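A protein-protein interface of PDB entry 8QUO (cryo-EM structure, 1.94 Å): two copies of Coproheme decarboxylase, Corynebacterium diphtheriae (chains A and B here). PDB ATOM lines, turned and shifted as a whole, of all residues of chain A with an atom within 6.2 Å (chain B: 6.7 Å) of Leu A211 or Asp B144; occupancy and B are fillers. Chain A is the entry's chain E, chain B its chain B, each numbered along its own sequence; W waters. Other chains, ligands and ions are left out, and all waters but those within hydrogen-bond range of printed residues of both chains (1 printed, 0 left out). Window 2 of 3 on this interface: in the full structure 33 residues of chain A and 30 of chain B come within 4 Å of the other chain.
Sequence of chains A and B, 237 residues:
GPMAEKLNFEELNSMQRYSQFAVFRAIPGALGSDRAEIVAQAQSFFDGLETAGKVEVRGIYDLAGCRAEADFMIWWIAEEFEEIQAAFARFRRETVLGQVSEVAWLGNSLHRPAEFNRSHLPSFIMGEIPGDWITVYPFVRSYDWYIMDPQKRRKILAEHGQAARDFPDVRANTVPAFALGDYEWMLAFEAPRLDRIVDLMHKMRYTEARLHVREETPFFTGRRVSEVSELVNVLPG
The backbone carbonyl oxygen of Val A213 lies close to the side-chain hydroxyl of Tyr B143 (3.4 Å).
The side-chain hydroxyl (OG) of Ser B142 is in hydrogen-bond range of the side-chain carboxylate (OD1) of Asp B144 (3.0 Å).
Ile B147 touches Thr A207 (CG2 to O, 3.2 Å).
CD1 of Tyr B143 touches O of Arg A210, 3.3 Å away.
Asp B144 touches Leu A211 (CB to CD2, 3.6 Å).
Leu A211 touches Ile B147 (CG to CD1, 3.6 Å).
Of the printed residues of chain A, Asp B144 touches Leu A211 (3.6 Å).
Printed residues of chain A within 4 Å of Tyr B143: Arg A210 and Val A213.
Printed residues of chain B within 4 Å of Val A213: Tyr B143 (3.4 Å).
Of the printed residues of chain A, Ile B147 touches Thr A207 and Leu A211.
Printed residues of chain B within 4 Å of Thr A207: Ile B147 (3.2 Å).
Printed residues of chain B within 4 Å of Arg A210: Tyr B143 (3.3 Å).
Ala A209 touches none of the printed residues of chain B.
The nearest residue of chain B that does not touch Leu A211 is Tyr B143 (4.4 Å).
Of the 8 printed residues of chain A, 4 touch a printed residue of chain B.
Printed residues of chain A that touch a printed residue of chain B: Thr A207, Arg A210, Leu A211 and Val A213.
Of the 12 printed residues of chain B, 3 touch a printed residue of chain A.
Printed residues of chain B that touch a printed residue of chain A: Tyr B143, Asp B144 and Ile B147.
Among the printed residues, no Asp or Glu carboxylate lies within 4 Å of a Lys or Arg side-chain nitrogen of the other chain.
Positions printed for both chains: 142, 211 and 212.
Of the 5 pairs that touch across the chains among the printed residues, none has its exchanged pair printed and touching as well.
Water W1 bridges the guanidinium group (NE) of Arg A210 (2.9 Å) and the backbone carbonyl oxygen (O) of Tyr B143 (3.0 Å).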
ATOM      1  N   SER A 142      10.598   0.345   1.835  1.00  0.00           N
ATOM      2  CA  SER A 142       9.225  -0.098   1.671  1.00  0.00           C
ATOM      3  C   SER A 142       8.329   0.554   2.720  1.00  0.00           C
ATOM      4  O   SER A 142       8.794   1.089   3.730  1.00  0.00           O
ATOM      5  CB  SER A 142       9.135  -1.620   1.767  1.00  0.00           C
ATOM      6  OG  SER A 142       9.444  -2.068   3.073  1.00  0.00           O
ATOM      7  N   THR A 207      21.196  -9.731  -0.207  1.00  0.00           N
ATOM      8  CA  THR A 207      20.794  -9.441   1.160  1.00  0.00           C
ATOM      9  C   THR A 207      19.277  -9.419   1.252  1.00  0.00           C
ATOM     10  O   THR A 207      18.585  -9.124   0.275  1.00  0.00           O
ATOM     11  CB  THR A 207      21.355  -8.099   1.653  1.00  0.00           C
ATOM     12  OG1 THR A 207      20.977  -7.058   0.744  1.00  0.00           O
ATOM     13  CG2 THR A 207      22.866  -8.151   1.751  1.00  0.00           C
ATOM     14  N   GLU A 208      18.768  -9.731   2.445  1.00  0.00           N
ATOM     15  CA  GLU A 208      17.326  -9.706   2.661  1.00  0.00           C
ATOM     16  C   GLU A 208      16.769  -8.291   2.587  1.00  0.00           C
ATOM     17  O   GLU A 208      15.590  -8.108   2.259  1.00  0.00           O
ATOM     18  CB  GLU A 208      16.990 -10.342   4.010  1.00  0.00           C
ATOM     19  CG  GLU A 208      15.512 -10.610   4.222  1.00  0.00           C
ATOM     20  CD  GLU A 208      15.230 -11.313   5.533  1.00  0.00           C
ATOM     21  OE1 GLU A 208      16.196 -11.663   6.242  1.00  0.00           O
ATOM     22  OE2 GLU A 208      14.041 -11.514   5.858  1.00  0.00           O
ATOM     23  N   ALA A 209      17.597  -7.281   2.870  1.00  0.00           N
ATOM     24  CA  ALA A 209      17.143  -5.896   2.808  1.00  0.00           C
ATOM     25  C   ALA A 209      16.646  -5.511   1.422  1.00  0.00           C
ATOM     26  O   ALA A 209      15.819  -4.601   1.303  1.00  0.00           O
ATOM     27  CB  ALA A 209      18.268  -4.956   3.240  1.00  0.00           C
ATOM     28  N   ARG A 210      17.115  -6.198   0.377  1.00  0.00           N
ATOM     29  CA  ARG A 210      16.638  -5.929  -0.975  1.00  0.00           C
ATOM     30  C   ARG A 210      15.146  -6.183  -1.119  1.00  0.00           C
ATOM     31  O   ARG A 210      14.532  -5.686  -2.070  1.00  0.00           O
ATOM     32  CB  ARG A 210      17.412  -6.779  -1.982  1.00  0.00           C
ATOM     33  CG  ARG A 210      18.903  -6.508  -2.005  1.00  0.00           C
ATOM     34  CD  ARG A 210      19.192  -5.073  -2.399  1.00  0.00           C
ATOM     35  NE  ARG A 210      18.571  -4.726  -3.669  1.00  0.00           N
ATOM     36  CZ  ARG A 210      18.510  -3.497  -4.163  1.00  0.00           C
ATOM     37  NH1 ARG A 210      19.028  -2.467  -3.516  1.00  0.00           N
ATOM     38  NH2 ARG A 210      17.917  -3.297  -5.335  1.00  0.00           N
ATOM     39  N   LEU A 211      14.547  -6.943  -0.204  1.00  0.00           N
ATOM     40  CA  LEU A 211      13.110  -7.172  -0.225  1.00  0.00           C
ATOM     41  C   LEU A 211      12.309  -5.972   0.259  1.00  0.00           C
ATOM     42  O   LEU A 211      11.077  -6.007   0.192  1.00  0.00           O
ATOM     43  CB  LEU A 211      12.758  -8.392   0.627  1.00  0.00           C
ATOM     44  CG  LEU A 211      13.257  -9.736   0.103  1.00  0.00           C
ATOM     45  CD1 LEU A 211      12.714 -10.879   0.939  1.00  0.00           C
ATOM     46  CD2 LEU A 211      12.875  -9.906  -1.356  1.00  0.00           C
ATOM     47  N   HIS A 212      12.967  -4.922   0.741  1.00  0.00           N
ATOM     48  CA  HIS A 212      12.290  -3.766   1.316  1.00  0.00           C
ATOM     49  C   HIS A 212      12.792  -2.479   0.676  1.00  0.00           C
ATOM     50  O   HIS A 212      13.134  -1.507   1.351  1.00  0.00           O
ATOM     51  CB  HIS A 212      12.477  -3.742   2.827  1.00  0.00           C
ATOM     52  CG  HIS A 212      12.155  -5.045   3.490  1.00  0.00           C
ATOM     53  ND1 HIS A 212      10.865  -5.446   3.756  1.00  0.00           N
ATOM     54  CD2 HIS A 212      12.958  -6.041   3.931  1.00  0.00           C
ATOM     55  CE1 HIS A 212      10.886  -6.632   4.336  1.00  0.00           C
ATOM     56  NE2 HIS A 212      12.144  -7.015   4.454  1.00  0.00           N
ATOM     57  N   VAL A 213      12.841  -2.462  -0.653  1.00  0.00           N
ATOM     58  CA  VAL A 213      13.314  -1.317  -1.419  1.00  0.00           C
ATOM     59  C   VAL A 213      12.179  -0.831  -2.308  1.00  0.00           C
ATOM     60  O   VAL A 213      11.505  -1.637  -2.957  1.00  0.00           O
ATOM     61  CB  VAL A 213      14.551  -1.674  -2.264  1.00  0.00           C
ATOM     62  CG1 VAL A 213      15.080  -0.443  -2.981  1.00  0.00           C
ATOM     63  CG2 VAL A 213      15.627  -2.295  -1.392  1.00  0.00           C
ATOM     64  N   ARG B 141      16.810  -6.900 -12.582  1.00  0.00           N
ATOM     65  CA  ARG B 141      16.146  -8.107 -12.124  1.00  0.00           C
ATOM     66  C   ARG B 141      15.167  -7.785 -10.997  1.00  0.00           C
ATOM     67  O   ARG B 141      15.121  -6.670 -10.474  1.00  0.00           O
ATOM     68  CB  ARG B 141      17.168  -9.139 -11.656  1.00  0.00           C
ATOM     69  CG  ARG B 141      17.875  -9.869 -12.779  1.00  0.00           C
ATOM     70  CD  ARG B 141      17.059 -11.050 -13.261  1.00  0.00           C
ATOM     71  NE  ARG B 141      17.700 -11.739 -14.374  1.00  0.00           N
ATOM     72  CZ  ARG B 141      17.046 -12.320 -15.369  1.00  0.00           C
ATOM     73  NH1 ARG B 141      15.726 -12.314 -15.423  1.00  0.00           N
ATOM     74  NH2 ARG B 141      17.734 -12.920 -16.334  1.00  0.00           N
ATOM     75  N   SER B 142      14.375  -8.785 -10.626  1.00  0.00           N
ATOM     76  CA  SER B 142      13.457  -8.630  -9.512  1.00  0.00           C
ATOM     77  C   SER B 142      14.229  -8.496  -8.202  1.00  0.00           C
ATOM     78  O   SER B 142      15.415  -8.821  -8.110  1.00  0.00           O
ATOM     79  CB  SER B 142      12.491  -9.811  -9.439  1.00  0.00           C
ATOM     80  OG  SER B 142      13.177 -11.015  -9.149  1.00  0.00           O
ATOM     81  N   TYR B 143      13.533  -8.002  -7.177  1.00  0.00           N
ATOM     82  CA  TYR B 143      14.186  -7.717  -5.903  1.00  0.00           C
ATOM     83  C   TYR B 143      14.710  -8.987  -5.245  1.00  0.00           C
ATOM     84  O   TYR B 143      15.784  -8.979  -4.634  1.00  0.00           O
ATOM     85  CB  TYR B 143      13.216  -6.992  -4.972  1.00  0.00           C
ATOM     86  CG  TYR B 143      13.044  -5.526  -5.291  1.00  0.00           C
ATOM     87  CD1 TYR B 143      14.115  -4.647  -5.209  1.00  0.00           C
ATOM     88  CD2 TYR B 143      11.811  -5.020  -5.673  1.00  0.00           C
ATOM     89  CE1 TYR B 143      13.961  -3.307  -5.498  1.00  0.00           C
ATOM     90  CE2 TYR B 143      11.648  -3.681  -5.964  1.00  0.00           C
ATOM     91  CZ  TYR B 143      12.725  -2.830  -5.875  1.00  0.00           C
ATOM     92  OH  TYR B 143      12.568  -1.495  -6.163  1.00  0.00           O
ATOM     93  N   ASP B 144      13.968 -10.086  -5.355  1.00  0.00           N
ATOM     94  CA  ASP B 144      14.325 -11.342  -4.709  1.00  0.00           C
ATOM     95  C   ASP B 144      15.167 -12.250  -5.596  1.00  0.00           C
ATOM     96  O   ASP B 144      15.421 -13.398  -5.219  1.00  0.00           O
ATOM     97  CB  ASP B 144      13.060 -12.081  -4.267  1.00  0.00           C
ATOM     98  CG  ASP B 144      12.255 -12.608  -5.436  1.00  0.00           C
ATOM     99  OD1 ASP B 144      12.266 -11.968  -6.507  1.00  0.00           O
ATOM    100  OD2 ASP B 144      11.608 -13.664  -5.284  1.00  0.00           O
ATOM    101  N   TRP B 145      15.595 -11.767  -6.763  1.00  0.00           N
ATOM    102  CA  TRP B 145      16.296 -12.623  -7.715  1.00  0.00           C
ATOM    103  C   TRP B 145      17.630 -13.112  -7.163  1.00  0.00           C
ATOM    104  O   TRP B 145      17.979 -14.287  -7.318  1.00  0.00           O
ATOM    105  CB  TRP B 145      16.502 -11.870  -9.028  1.00  0.00           C
ATOM    106  CG  TRP B 145      17.460 -12.519  -9.974  1.00  0.00           C
ATOM    107  CD1 TRP B 145      18.742 -12.137 -10.227  1.00  0.00           C
ATOM    108  CD2 TRP B 145      17.207 -13.654 -10.809  1.00  0.00           C
ATOM    109  NE1 TRP B 145      19.308 -12.966 -11.162  1.00  0.00           N
ATOM    110  CE2 TRP B 145      18.385 -13.906 -11.536  1.00  0.00           C
ATOM    111  CE3 TRP B 145      16.101 -14.484 -11.009  1.00  0.00           C
ATOM    112  CZ2 TRP B 145      18.488 -14.951 -12.449  1.00  0.00           C
ATOM    113  CZ3 TRP B 145      16.206 -15.519 -11.914  1.00  0.00           C
ATOM    114  CH2 TRP B 145      17.390 -15.745 -12.622  1.00  0.00           C
ATOM    115  N   TYR B 146      18.388 -12.229  -6.512  1.00  0.00           N
ATOM    116  CA  TYR B 146      19.735 -12.581  -6.082  1.00  0.00           C
ATOM    117  C   TYR B 146      19.766 -13.344  -4.765  1.00  0.00           C
ATOM    118  O   TYR B 146      20.730 -14.073  -4.515  1.00  0.00           O
ATOM    119  CB  TYR B 146      20.596 -11.322  -5.979  1.00  0.00           C
ATOM    120  CG  TYR B 146      20.693 -10.563  -7.281  1.00  0.00           C
ATOM    121  CD1 TYR B 146      21.663 -10.881  -8.220  1.00  0.00           C
ATOM    122  CD2 TYR B 146      19.810  -9.534  -7.575  1.00  0.00           C
ATOM    123  CE1 TYR B 146      21.753 -10.193  -9.413  1.00  0.00           C
ATOM    124  CE2 TYR B 146      19.893  -8.841  -8.763  1.00  0.00           C
ATOM    125  CZ  TYR B 146      20.866  -9.175  -9.678  1.00  0.00           C
ATOM    126  OH  TYR B 146      20.949  -8.485 -10.864  1.00  0.00           O
ATOM    127  N   ILE B 147      18.742 -13.201  -3.917  1.00  0.00           N
ATOM    128  CA  ILE B 147      18.677 -13.976  -2.682  1.00  0.00           C
ATOM    129  C   ILE B 147      17.904 -15.272  -2.856  1.00  0.00           C
ATOM    130  O   ILE B 147      17.751 -16.027  -1.886  1.00  0.00           O
ATOM    131  CB  ILE B 147      18.058 -13.154  -1.535  1.00  0.00           C
ATOM    132  CG1 ILE B 147      16.628 -12.744  -1.883  1.00  0.00           C
ATOM    133  CG2 ILE B 147      18.912 -11.939  -1.242  1.00  0.00           C
ATOM    134  CD1 ILE B 147      16.061 -11.713  -0.952  1.00  0.00           C
ATOM    135  N   MET B 148      17.408 -15.550  -4.058  1.00  0.00           N
ATOM    136  CA  MET B 148      16.793 -16.836  -4.345  1.00  0.00           C
ATOM    137  C   MET B 148      17.823 -17.949  -4.185  1.00  0.00           C
ATOM    138  O   MET B 148      19.023 -17.742  -4.381  1.00  0.00           O
ATOM    139  CB  MET B 148      16.213 -16.824  -5.763  1.00  0.00           C
ATOM    140  CG  MET B 148      16.030 -18.184  -6.416  1.00  0.00           C
ATOM    141  SD  MET B 148      15.408 -18.082  -8.105  1.00  0.00           S
ATOM    142  CE  MET B 148      14.634 -16.468  -8.095  1.00  0.00           C
ATOM    143  N   ASP B 149      17.344 -19.130  -3.779  1.00  0.00           N
ATOM    144  CA  ASP B 149      18.145 -20.342  -3.642  1.00  0.00           C
ATOM    145  C   ASP B 149      19.094 -20.479  -4.826  1.00  0.00           C
ATOM    146  O   ASP B 149      18.645 -20.505  -5.978  1.00  0.00           O
ATOM    147  CB  ASP B 149      17.233 -21.566  -3.536  1.00  0.00           C
ATOM    148  CG  ASP B 149      17.997 -22.856  -3.307  1.00  0.00           C
ATOM    149  OD1 ASP B 149      19.169 -22.798  -2.883  1.00  0.00           O
ATOM    150  OD2 ASP B 149      17.422 -23.934  -3.555  1.00  0.00           O
ATOM    151  N   ARG B 153      18.108 -20.586  -8.942  1.00  0.00           N
ATOM    152  CA  ARG B 153      18.523 -19.559  -9.892  1.00  0.00           C
ATOM    153  C   ARG B 153      19.443 -20.138 -10.958  1.00  0.00           C
ATOM    154  O   ARG B 153      19.359 -19.762 -12.132  1.00  0.00           O
ATOM    155  CB  ARG B 153      19.208 -18.409  -9.155  1.00  0.00           C
ATOM    156  CG  ARG B 153      19.612 -17.254 -10.055  1.00  0.00           C
ATOM    157  CD  ARG B 153      20.087 -16.049  -9.259  1.00  0.00           C
ATOM    158  NE  ARG B 153      21.275 -16.339  -8.468  1.00  0.00           N
ATOM    159  CZ  ARG B 153      21.273 -16.535  -7.157  1.00  0.00           C
ATOM    160  NH1 ARG B 153      20.156 -16.477  -6.452  1.00  0.00           N
ATOM    161  NH2 ARG B 153      22.420 -16.798  -6.538  1.00  0.00           N
ATOM    162  N   LEU B 211       9.807 -14.320 -15.269  1.00  0.00           N
ATOM    163  CA  LEU B 211       9.087 -14.062 -14.032  1.00  0.00           C
ATOM    164  C   LEU B 211       9.873 -13.201 -13.055  1.00  0.00           C
ATOM    165  O   LEU B 211       9.332 -12.832 -12.008  1.00  0.00           O
ATOM    166  CB  LEU B 211       8.715 -15.381 -13.354  1.00  0.00           C
ATOM    167  CG  LEU B 211       7.673 -16.236 -14.071  1.00  0.00           C
ATOM    168  CD1 LEU B 211       7.241 -17.402 -13.201  1.00  0.00           C
ATOM    169  CD2 LEU B 211       6.479 -15.388 -14.468  1.00  0.00           C
ATOM    170  N   HIS B 212      11.124 -12.873 -13.362  1.00  0.00           N
ATOM    171  CA  HIS B 212      11.992 -12.138 -12.449  1.00  0.00           C
ATOM    172  C   HIS B 212      12.603 -10.932 -13.146  1.00  0.00           C
ATOM    173  O   HIS B 212      13.807 -10.682 -13.079  1.00  0.00           O
ATOM    174  CB  HIS B 212      13.066 -13.062 -11.889  1.00  0.00           C
ATOM    175  CG  HIS B 212      12.520 -14.326 -11.302  1.00  0.00           C
ATOM    176  ND1 HIS B 212      12.048 -14.402 -10.010  1.00  0.00           N
ATOM    177  CD2 HIS B 212      12.359 -15.559 -11.835  1.00  0.00           C
ATOM    178  CE1 HIS B 212      11.626 -15.630  -9.769  1.00  0.00           C
ATOM    179  NE2 HIS B 212      11.804 -16.352 -10.860  1.00  0.00           N
HETATM  180  O   HOH W   1      17.556  -6.734  -5.509  1.00  0.00           O
